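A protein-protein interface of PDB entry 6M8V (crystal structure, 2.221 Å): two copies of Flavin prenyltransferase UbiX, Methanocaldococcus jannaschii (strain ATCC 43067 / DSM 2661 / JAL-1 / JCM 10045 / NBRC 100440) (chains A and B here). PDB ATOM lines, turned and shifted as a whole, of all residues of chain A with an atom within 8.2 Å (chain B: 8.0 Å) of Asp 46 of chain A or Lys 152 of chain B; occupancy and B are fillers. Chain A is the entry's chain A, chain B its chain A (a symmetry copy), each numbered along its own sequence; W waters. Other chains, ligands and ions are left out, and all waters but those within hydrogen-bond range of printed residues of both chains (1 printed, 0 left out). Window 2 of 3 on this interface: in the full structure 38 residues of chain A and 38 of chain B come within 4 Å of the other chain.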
ATOM      1  N   SER A  11      -0.450   4.020 -11.090  1.00  0.00           N
ATOM      2  CA  SER A  11      -0.433   2.853 -11.958  1.00  0.00           C
ATOM      3  C   SER A  11      -1.398   1.792 -11.442  1.00  0.00           C
ATOM      4  O   SER A  11      -1.641   1.671 -10.238  1.00  0.00           O
ATOM      5  CB  SER A  11       0.981   2.276 -12.052  1.00  0.00           C
ATOM      6  OG  SER A  11       1.044   1.250 -13.031  1.00  0.00           O
ATOM      7  N   VAL A  13      -4.703   1.259 -13.025  1.00  0.00           N
ATOM      8  CA  VAL A  13      -6.107   1.581 -13.244  1.00  0.00           C
ATOM      9  C   VAL A  13      -6.897   0.402 -13.792  1.00  0.00           C
ATOM     10  O   VAL A  13      -8.133   0.447 -13.794  1.00  0.00           O
ATOM     11  CB  VAL A  13      -6.242   2.791 -14.191  1.00  0.00           C
ATOM     12  CG1 VAL A  13      -5.877   4.079 -13.461  1.00  0.00           C
ATOM     13  CG2 VAL A  13      -5.370   2.604 -15.425  1.00  0.00           C
ATOM     14  N   LYS A  39      -5.250  10.581 -17.886  1.00  0.00           N
ATOM     15  CA  LYS A  39      -4.049  10.334 -18.679  1.00  0.00           C
ATOM     16  C   LYS A  39      -3.505   8.928 -18.464  1.00  0.00           C
ATOM     17  O   LYS A  39      -2.973   8.324 -19.399  1.00  0.00           O
ATOM     18  CB  LYS A  39      -2.978  11.373 -18.349  1.00  0.00           C
ATOM     19  CG  LYS A  39      -3.393  12.805 -18.638  1.00  0.00           C
ATOM     20  CD  LYS A  39      -2.587  13.788 -17.806  1.00  0.00           C
ATOM     21  CE  LYS A  39      -3.038  15.222 -18.043  1.00  0.00           C
ATOM     22  NZ  LYS A  39      -2.449  16.145 -17.030  1.00  0.00           N
ATOM     23  N   ILE A  40      -3.633   8.383 -17.252  1.00  0.00           N
ATOM     24  CA  ILE A  40      -3.079   7.059 -16.989  1.00  0.00           C
ATOM     25  C   ILE A  40      -3.940   5.975 -17.632  1.00  0.00           C
ATOM     26  O   ILE A  40      -3.419   4.983 -18.156  1.00  0.00           O
ATOM     27  CB  ILE A  40      -2.908   6.848 -15.473  1.00  0.00           C
ATOM     28  CG1 ILE A  40      -1.811   7.780 -14.953  1.00  0.00           C
ATOM     29  CG2 ILE A  40      -2.569   5.398 -15.158  1.00  0.00           C
ATOM     30  CD1 ILE A  40      -1.279   7.422 -13.589  1.00  0.00           C
ATOM     31  N   ILE A  41      -5.265   6.144 -17.602  1.00  0.00           N
ATOM     32  CA  ILE A  41      -6.157   5.238 -18.327  1.00  0.00           C
ATOM     33  C   ILE A  41      -5.767   5.186 -19.800  1.00  0.00           C
ATOM     34  O   ILE A  41      -5.697   4.112 -20.411  1.00  0.00           O
ATOM     35  CB  ILE A  41      -7.621   5.680 -18.159  1.00  0.00           C
ATOM     36  CG1 ILE A  41      -8.094   5.486 -16.716  1.00  0.00           C
ATOM     37  CG2 ILE A  41      -8.528   4.929 -19.130  1.00  0.00           C
ATOM     38  CD1 ILE A  41      -9.415   6.164 -16.438  1.00  0.00           C
ATOM     39  N   LYS A  42      -5.507   6.354 -20.390  1.00  0.00           N
ATOM     40  CA  LYS A  42      -5.114   6.410 -21.796  1.00  0.00           C
ATOM     41  C   LYS A  42      -3.777   5.713 -22.025  1.00  0.00           C
ATOM     42  O   LYS A  42      -3.617   4.968 -22.998  1.00  0.00           O
ATOM     43  CB  LYS A  42      -5.053   7.869 -22.257  1.00  0.00           C
ATOM     44  CG  LYS A  42      -4.279   8.121 -23.546  1.00  0.00           C
ATOM     45  CD  LYS A  42      -4.793   7.305 -24.727  1.00  0.00           C
ATOM     46  CE  LYS A  42      -6.147   7.797 -25.209  1.00  0.00           C
ATOM     47  NZ  LYS A  42      -6.958   6.687 -25.781  1.00  0.00           N
ATOM     48  N   GLU A  43      -2.811   5.930 -21.131  1.00  0.00           N
ATOM     49  CA  GLU A  43      -1.474   5.390 -21.351  1.00  0.00           C
ATOM     50  C   GLU A  43      -1.406   3.896 -21.060  1.00  0.00           C
ATOM     51  O   GLU A  43      -0.755   3.151 -21.798  1.00  0.00           O
ATOM     52  CB  GLU A  43      -0.459   6.143 -20.493  1.00  0.00           C
ATOM     53  CG  GLU A  43       0.988   5.886 -20.885  1.00  0.00           C
ATOM     54  CD  GLU A  43       1.395   6.623 -22.149  1.00  0.00           C
ATOM     55  OE1 GLU A  43       0.535   7.300 -22.759  1.00  0.00           O
ATOM     56  OE2 GLU A  43       2.580   6.527 -22.531  1.00  0.00           O
ATOM     57  N   GLU A  44      -2.066   3.441 -19.999  1.00  0.00           N
ATOM     58  CA  GLU A  44      -1.945   2.055 -19.567  1.00  0.00           C
ATOM     59  C   GLU A  44      -2.993   1.140 -20.184  1.00  0.00           C
ATOM     60  O   GLU A  44      -2.732  -0.057 -20.355  1.00  0.00           O
ATOM     61  CB  GLU A  44      -2.040   1.962 -18.037  1.00  0.00           C
ATOM     62  CG  GLU A  44      -0.812   2.477 -17.297  1.00  0.00           C
ATOM     63  CD  GLU A  44      -0.841   2.153 -15.808  1.00  0.00           C
ATOM     64  OE1 GLU A  44      -1.890   1.690 -15.306  1.00  0.00           O
ATOM     65  OE2 GLU A  44       0.189   2.363 -15.138  1.00  0.00           O
ATOM     66  N   LEU A  45      -4.175   1.659 -20.498  1.00  0.00           N
ATOM     67  CA  LEU A  45      -5.244   0.849 -21.060  1.00  0.00           C
ATOM     68  C   LEU A  45      -5.479   1.127 -22.540  1.00  0.00           C
ATOM     69  O   LEU A  45      -6.323   0.466 -23.154  1.00  0.00           O
ATOM     70  CB  LEU A  45      -6.537   1.069 -20.267  1.00  0.00           C
ATOM     71  CG  LEU A  45      -6.456   0.637 -18.800  1.00  0.00           C
ATOM     72  CD1 LEU A  45      -7.776   0.860 -18.076  1.00  0.00           C
ATOM     73  CD2 LEU A  45      -6.027  -0.818 -18.702  1.00  0.00           C
ATOM     74  N   ASP A  46      -4.754   2.091 -23.120  1.00  0.00           N
ATOM     75  CA  ASP A  46      -4.819   2.413 -24.549  1.00  0.00           C
ATOM     76  C   ASP A  46      -6.253   2.636 -25.020  1.00  0.00           C
ATOM     77  O   ASP A  46      -6.584   2.429 -26.191  1.00  0.00           O
ATOM     78  CB  ASP A  46      -4.124   1.342 -25.392  1.00  0.00           C
ATOM     79  CG  ASP A  46      -2.612   1.383 -25.247  1.00  0.00           C
ATOM     80  OD1 ASP A  46      -2.000   0.311 -25.053  1.00  0.00           O
ATOM     81  OD2 ASP A  46      -2.037   2.492 -25.315  1.00  0.00           O
ATOM     82  N   ILE A  47      -7.113   3.063 -24.101  1.00  0.00           N
ATOM     83  CA  ILE A  47      -8.476   3.460 -24.408  1.00  0.00           C
ATOM     84  C   ILE A  47      -8.693   4.846 -23.825  1.00  0.00           C
ATOM     85  O   ILE A  47      -8.053   5.234 -22.842  1.00  0.00           O
ATOM     86  CB  ILE A  47      -9.515   2.465 -23.847  1.00  0.00           C
ATOM     87  CG1 ILE A  47      -9.375   2.352 -22.329  1.00  0.00           C
ATOM     88  CG2 ILE A  47      -9.362   1.107 -24.507  1.00  0.00           C
ATOM     89  CD1 ILE A  47     -10.594   1.783 -21.640  1.00  0.00           C
ATOM     90  N   ASP A  48      -9.595   5.600 -24.441  1.00  0.00           N
ATOM     91  CA  ASP A  48      -9.915   6.916 -23.916  1.00  0.00           C
ATOM     92  C   ASP A  48     -10.677   6.786 -22.601  1.00  0.00           C
ATOM     93  O   ASP A  48     -11.397   5.810 -22.370  1.00  0.00           O
ATOM     94  CB  ASP A  48     -10.728   7.715 -24.930  1.00  0.00           C
ATOM     95  CG  ASP A  48     -10.975   9.133 -24.476  1.00  0.00           C
ATOM     96  OD1 ASP A  48     -10.057   9.972 -24.610  1.00  0.00           O
ATOM     97  OD2 ASP A  48     -12.084   9.403 -23.976  1.00  0.00           O
ATOM     98  N   TRP A  49     -10.501   7.781 -21.725  1.00  0.00           N
ATOM     99  CA  TRP A  49     -11.078   7.692 -20.388  1.00  0.00           C
ATOM    100  C   TRP A  49     -12.601   7.637 -20.423  1.00  0.00           C
ATOM    101  O   TRP A  49     -13.216   7.023 -19.544  1.00  0.00           O
ATOM    102  CB  TRP A  49     -10.606   8.865 -19.528  1.00  0.00           C
ATOM    103  CG  TRP A  49     -11.224  10.188 -19.877  1.00  0.00           C
ATOM    104  CD1 TRP A  49     -10.749  11.107 -20.771  1.00  0.00           C
ATOM    105  CD2 TRP A  49     -12.420  10.751 -19.323  1.00  0.00           C
ATOM    106  NE1 TRP A  49     -11.579  12.202 -20.809  1.00  0.00           N
ATOM    107  CE2 TRP A  49     -12.613  12.008 -19.933  1.00  0.00           C
ATOM    108  CE3 TRP A  49     -13.348  10.313 -18.372  1.00  0.00           C
ATOM    109  CZ2 TRP A  49     -13.695  12.830 -19.622  1.00  0.00           C
ATOM    110  CZ3 TRP A  49     -14.423  11.128 -18.068  1.00  0.00           C
ATOM    111  CH2 TRP A  49     -14.587  12.373 -18.690  1.00  0.00           C
ATOM    112  N   GLU A  51     -14.373   5.868 -22.131  1.00  0.00           N
ATOM    113  CA  GLU A  51     -14.776   4.465 -22.182  1.00  0.00           C
ATOM    114  C   GLU A  51     -15.009   3.897 -20.789  1.00  0.00           C
ATOM    115  O   GLU A  51     -15.835   2.997 -20.617  1.00  0.00           O
ATOM    116  CB  GLU A  51     -13.712   3.639 -22.904  1.00  0.00           C
ATOM    117  CG  GLU A  51     -13.740   3.732 -24.424  1.00  0.00           C
ATOM    118  CD  GLU A  51     -14.850   2.906 -25.042  1.00  0.00           C
ATOM    119  OE1 GLU A  51     -15.956   3.450 -25.256  1.00  0.00           O
ATOM    120  OE2 GLU A  51     -14.614   1.708 -25.313  1.00  0.00           O
ATOM    121  N   VAL A 156      -2.388 -12.531 -16.305  1.00  0.00           N
ATOM    122  CA  VAL A 156      -2.606 -11.240 -15.660  1.00  0.00           C
ATOM    123  C   VAL A 156      -4.042 -11.128 -15.166  1.00  0.00           C
ATOM    124  O   VAL A 156      -4.300 -10.632 -14.063  1.00  0.00           O
ATOM    125  CB  VAL A 156      -2.251 -10.101 -16.632  1.00  0.00           C
ATOM    126  CG1 VAL A 156      -2.669  -8.757 -16.058  1.00  0.00           C
ATOM    127  CG2 VAL A 156      -0.764 -10.122 -16.949  1.00  0.00           C
ATOM    128  N   ALA B 148       3.166  -2.490 -10.676  1.00  0.00           N
ATOM    129  CA  ALA B 148       2.597  -1.446 -11.513  1.00  0.00           C
ATOM    130  C   ALA B 148       2.275  -2.023 -12.888  1.00  0.00           C
ATOM    131  O   ALA B 148       2.598  -3.171 -13.198  1.00  0.00           O
ATOM    132  CB  ALA B 148       3.558  -0.264 -11.634  1.00  0.00           C
ATOM    133  N   PHE B 149       1.629  -1.209 -13.722  1.00  0.00           N
ATOM    134  CA  PHE B 149       1.186  -1.673 -15.030  1.00  0.00           C
ATOM    135  C   PHE B 149       1.545  -0.712 -16.158  1.00  0.00           C
ATOM    136  O   PHE B 149       1.063  -0.895 -17.282  1.00  0.00           O
ATOM    137  CB  PHE B 149      -0.329  -1.930 -15.023  1.00  0.00           C
ATOM    138  CG  PHE B 149      -0.749  -3.056 -14.116  1.00  0.00           C
ATOM    139  CD1 PHE B 149      -0.905  -2.848 -12.751  1.00  0.00           C
ATOM    140  CD2 PHE B 149      -0.988  -4.323 -14.625  1.00  0.00           C
ATOM    141  CE1 PHE B 149      -1.287  -3.882 -11.910  1.00  0.00           C
ATOM    142  CE2 PHE B 149      -1.373  -5.364 -13.789  1.00  0.00           C
ATOM    143  CZ  PHE B 149      -1.520  -5.143 -12.429  1.00  0.00           C
ATOM    144  N   TYR B 150       2.375   0.306 -15.900  1.00  0.00           N
ATOM    145  CA  TYR B 150       2.788   1.185 -16.989  1.00  0.00           C
ATOM    146  C   TYR B 150       3.729   0.487 -17.961  1.00  0.00           C
ATOM    147  O   TYR B 150       3.890   0.957 -19.092  1.00  0.00           O
ATOM    148  CB  TYR B 150       3.440   2.467 -16.451  1.00  0.00           C
ATOM    149  CG  TYR B 150       4.545   2.282 -15.428  1.00  0.00           C
ATOM    150  CD1 TYR B 150       5.818   1.858 -15.807  1.00  0.00           C
ATOM    151  CD2 TYR B 150       4.325   2.568 -14.084  1.00  0.00           C
ATOM    152  CE1 TYR B 150       6.830   1.704 -14.873  1.00  0.00           C
ATOM    153  CE2 TYR B 150       5.329   2.418 -13.145  1.00  0.00           C
ATOM    154  CZ  TYR B 150       6.579   1.987 -13.542  1.00  0.00           C
ATOM    155  OH  TYR B 150       7.574   1.841 -12.603  1.00  0.00           O
ATOM    156  N   ASN B 151       4.348  -0.620 -17.548  1.00  0.00           N
ATOM    157  CA  ASN B 151       5.133  -1.455 -18.448  1.00  0.00           C
ATOM    158  C   ASN B 151       4.270  -2.392 -19.281  1.00  0.00           C
ATOM    159  O   ASN B 151       4.815  -3.142 -20.098  1.00  0.00           O
ATOM    160  CB  ASN B 151       6.166  -2.269 -17.657  1.00  0.00           C
ATOM    161  CG  ASN B 151       5.536  -3.119 -16.560  1.00  0.00           C
ATOM    162  OD1 ASN B 151       4.586  -2.699 -15.899  1.00  0.00           O
ATOM    163  ND2 ASN B 151       6.068  -4.320 -16.365  1.00  0.00           N
ATOM    164  N   LYS B 152       2.948  -2.359 -19.091  1.00  0.00           N
ATOM    165  CA  LYS B 152       1.978  -3.181 -19.806  1.00  0.00           C
ATOM    166  C   LYS B 152       2.388  -4.648 -19.772  1.00  0.00           C
ATOM    167  O   LYS B 152       2.845  -5.188 -20.787  1.00  0.00           O
ATOM    168  CB  LYS B 152       1.824  -2.702 -21.248  1.00  0.00           C
ATOM    169  CG  LYS B 152       1.357  -1.262 -21.372  1.00  0.00           C
ATOM    170  CD  LYS B 152       0.975  -0.935 -22.803  1.00  0.00           C
ATOM    171  CE  LYS B 152       0.320   0.431 -22.901  1.00  0.00           C
ATOM    172  NZ  LYS B 152       1.262   1.494 -23.361  1.00  0.00           N
ATOM    173  N   PRO B 153       2.244  -5.318 -18.632  1.00  0.00           N
ATOM    174  CA  PRO B 153       2.618  -6.735 -18.566  1.00  0.00           C
ATOM    175  C   PRO B 153       1.719  -7.577 -19.455  1.00  0.00           C
ATOM    176  O   PRO B 153       0.507  -7.365 -19.526  1.00  0.00           O
ATOM    177  CB  PRO B 153       2.427  -7.084 -17.086  1.00  0.00           C
ATOM    178  CG  PRO B 153       1.422  -6.089 -16.598  1.00  0.00           C
ATOM    179  CD  PRO B 153       1.692  -4.825 -17.359  1.00  0.00           C
ATOM    180  N   LYS B 154       2.335  -8.533 -20.149  1.00  0.00           N
ATOM    181  CA  LYS B 154       1.606  -9.445 -21.016  1.00  0.00           C
ATOM    182  C   LYS B 154       1.286 -10.770 -20.341  1.00  0.00           C
ATOM    183  O   LYS B 154       0.471 -11.536 -20.866  1.00  0.00           O
ATOM    184  CB  LYS B 154       2.401  -9.702 -22.302  1.00  0.00           C
ATOM    185  CG  LYS B 154       2.552  -8.475 -23.185  1.00  0.00           C
ATOM    186  CD  LYS B 154       1.242  -7.706 -23.263  1.00  0.00           C
ATOM    187  CE  LYS B 154       1.238  -6.706 -24.405  1.00  0.00           C
ATOM    188  NZ  LYS B 154      -0.065  -5.989 -24.487  1.00  0.00           N
ATOM    189  N   ASN B 155       1.891 -11.049 -19.193  1.00  0.00           N
ATOM    190  CA  ASN B 155       1.712 -12.328 -18.523  1.00  0.00           C
ATOM    191  C   ASN B 155       2.135 -12.168 -17.074  1.00  0.00           C
ATOM    192  O   ASN B 155       2.670 -11.132 -16.673  1.00  0.00           O
ATOM    193  CB  ASN B 155       2.526 -13.428 -19.203  1.00  0.00           C
ATOM    194  CG  ASN B 155       3.911 -12.959 -19.591  1.00  0.00           C
ATOM    195  OD1 ASN B 155       4.699 -12.551 -18.739  1.00  0.00           O
ATOM    196  ND2 ASN B 155       4.217 -13.011 -20.884  1.00  0.00           N
ATOM    197  N   ASP B 158       5.824 -11.163 -16.547  1.00  0.00           N
ATOM    198  CA  ASP B 158       6.163  -9.743 -16.627  1.00  0.00           C
ATOM    199  C   ASP B 158       5.895  -9.025 -15.309  1.00  0.00           C
ATOM    200  O   ASP B 158       6.602  -8.074 -14.960  1.00  0.00           O
ATOM    201  CB  ASP B 158       5.367  -9.064 -17.739  1.00  0.00           C
ATOM    202  CG  ASP B 158       5.838  -9.452 -19.127  1.00  0.00           C
ATOM    203  OD1 ASP B 158       7.012  -9.852 -19.283  1.00  0.00           O
ATOM    204  OD2 ASP B 158       5.020  -9.345 -20.064  1.00  0.00           O
ATOM    205  N   ILE B 159       4.864  -9.447 -14.583  1.00  0.00           N
ATOM    206  CA  ILE B 159       4.583  -8.852 -13.286  1.00  0.00           C
ATOM    207  C   ILE B 159       5.668  -9.229 -12.287  1.00  0.00           C
ATOM    208  O   ILE B 159       6.171  -8.375 -11.546  1.00  0.00           O
ATOM    209  CB  ILE B 159       3.184  -9.278 -12.813  1.00  0.00           C
ATOM    210  CG1 ILE B 159       2.123  -8.687 -13.748  1.00  0.00           C
ATOM    211  CG2 ILE B 159       2.955  -8.868 -11.367  1.00  0.00           C
ATOM    212  CD1 ILE B 159       0.711  -8.938 -13.308  1.00  0.00           C
ATOM    213  N   PHE B 162       8.889  -7.282 -12.980  1.00  0.00           N
ATOM    214  CA  PHE B 162       8.835  -5.895 -12.525  1.00  0.00           C
ATOM    215  C   PHE B 162       9.202  -5.795 -11.050  1.00  0.00           C
ATOM    216  O   PHE B 162      10.067  -4.998 -10.660  1.00  0.00           O
ATOM    217  CB  PHE B 162       7.442  -5.305 -12.768  1.00  0.00           C
ATOM    218  CG  PHE B 162       7.275  -3.909 -12.224  1.00  0.00           C
ATOM    219  CD1 PHE B 162       7.559  -2.809 -13.013  1.00  0.00           C
ATOM    220  CD2 PHE B 162       6.847  -3.697 -10.918  1.00  0.00           C
ATOM    221  CE1 PHE B 162       7.418  -1.528 -12.518  1.00  0.00           C
ATOM    222  CE2 PHE B 162       6.709  -2.419 -10.415  1.00  0.00           C
ATOM    223  CZ  PHE B 162       6.994  -1.332 -11.218  1.00  0.00           C
ATOM    224  N   LYS B 179      10.380  -2.964 -18.495  1.00  0.00           N
ATOM    225  CA  LYS B 179      10.341  -1.736 -19.281  1.00  0.00           C
ATOM    226  C   LYS B 179      10.088  -0.563 -18.343  1.00  0.00           C
ATOM    227  O   LYS B 179       8.996  -0.435 -17.779  1.00  0.00           O
ATOM    228  CB  LYS B 179       9.263  -1.828 -20.357  1.00  0.00           C
ATOM    229  CG  LYS B 179       9.375  -3.063 -21.234  1.00  0.00           C
ATOM    230  CD  LYS B 179       8.157  -3.222 -22.131  1.00  0.00           C
ATOM    231  CE  LYS B 179       8.298  -4.437 -23.037  1.00  0.00           C
ATOM    232  NZ  LYS B 179       9.511  -4.350 -23.896  1.00  0.00           N
ATOM    233  N   THR B 183      10.231   4.196 -20.777  1.00  0.00           N
ATOM    234  CA  THR B 183      10.252   3.158 -21.806  1.00  0.00           C
ATOM    235  C   THR B 183      11.655   2.997 -22.376  1.00  0.00           C
ATOM    236  O   THR B 183      12.550   2.493 -21.694  1.00  0.00           O
ATOM    237  CB  THR B 183       9.248   3.447 -22.949  1.00  0.00           C
ATOM    238  OG1 THR B 183       9.636   4.635 -23.651  1.00  0.00           O
ATOM    239  CG2 THR B 183       7.839   3.623 -22.396  1.00  0.00           C
HETATM  240  O   HOH W   1      -1.917 -12.434 -19.299  1.00  0.00           O
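No position is printed for both chains.
Lys 39 of chain A touches none of the printed residues of chain B.
Of the printed residues of chain B, Glu 44 of chain A touches Phe 149 (3.5 Å) and Tyr 150 (3.1 Å).
Of the printed residues of chain B, Val 156 of chain A touches Pro 153 (3.98 Å) and Asn 155 (3.6 Å).
Of the printed residues of chain A, Ala 148 of chain B touches Ser 11.
Of the printed residues of chain A, Phe 149 of chain B touches Ser 11 (2.6 Å) and Glu 44 (3.5 Å).
Of the printed residues of chain A, Lys 152 of chain B touches Glu 43 and Asp 46.
Of the printed residues of chain A, Asn 155 of chain B touches Val 156 (3.6 Å).
The nearest printed residue of chain B that does not touch Ser 11 of chain A is Asn 151 of chain B (5.9 Å).
Ser 11 of chain A touches Ala 148 of chain B (OG to CB, 3.3 Å).
Phe 149 of chain B touches Glu 44 of chain A.
Pro 153 of chain B touches Val 156 of chain A.
Asn 155 of chain B touches Val 156 of chain A.
The side-chain carboxylate of Glu 44 of chain A sits at hydrogen-bond distance from the side-chain hydroxyl of Ser 11 of chain A, 2.5 Å away.
The side-chain amide oxygen (OD1) of Asn 155 of chain B is in hydrogen-bond range of the backbone NH (N) of Asp 158 of chain B, at 2.8 Å.
O of Ala 148 of chain B lies close to OD1 of Asn 151 of chain B, 3.4 Å away.
Of the 13 printed residues of chain B, 6 touch a printed residue of chain A.
Hydrophobic or aromatic side chains of chain B within 4 Å of the printed part of chain A: Ala 148, Phe 149 and Tyr 150.
Along chain B the printed residues that touch a printed residue of chain A span positions 148 to 155.
Printed residues of chain A that touch a printed residue of chain B: Ser 11, Glu 43, Glu 44, Asp 46 and Val 156.
Hydrophobic or aromatic side chains of chain A within 4 Å of the printed part of chain B: Val 156.
Along chain A the printed residues that touch a printed residue of chain B span positions 11 to 156.
Among the printed residues, 9 pairs touch across the chains.
Water W1 lies within hydrogen-bond range of the backbone carbonyl oxygen (O) of Lys 154 of chain B (3.0 Å) and the backbone NH (N) of Val 156 of chain A (3.0 Å).
OG of Ser 11 of chain A lies within hydrogen-bond range of N of Phe 149 of chain B, 2.6 Å away.
The side-chain carboxylate (OD1) of Asp 46 of chain A lies within salt-bridge range of the side-chain amino group (NZ) of Lys 152 of chain B.
OG of Ser 11 of chain A is in hydrogen-bond range of N of Tyr 150 of chain B (3.3 Å).
NZ of Lys 152 of chain B is in hydrogen-bond range of O of Glu 43 of chain A, 3.0 Å away.
The side-chain carboxylate of Glu 44 of chain A is in hydrogen-bond range of the backbone NH of Tyr 150 of chain B.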
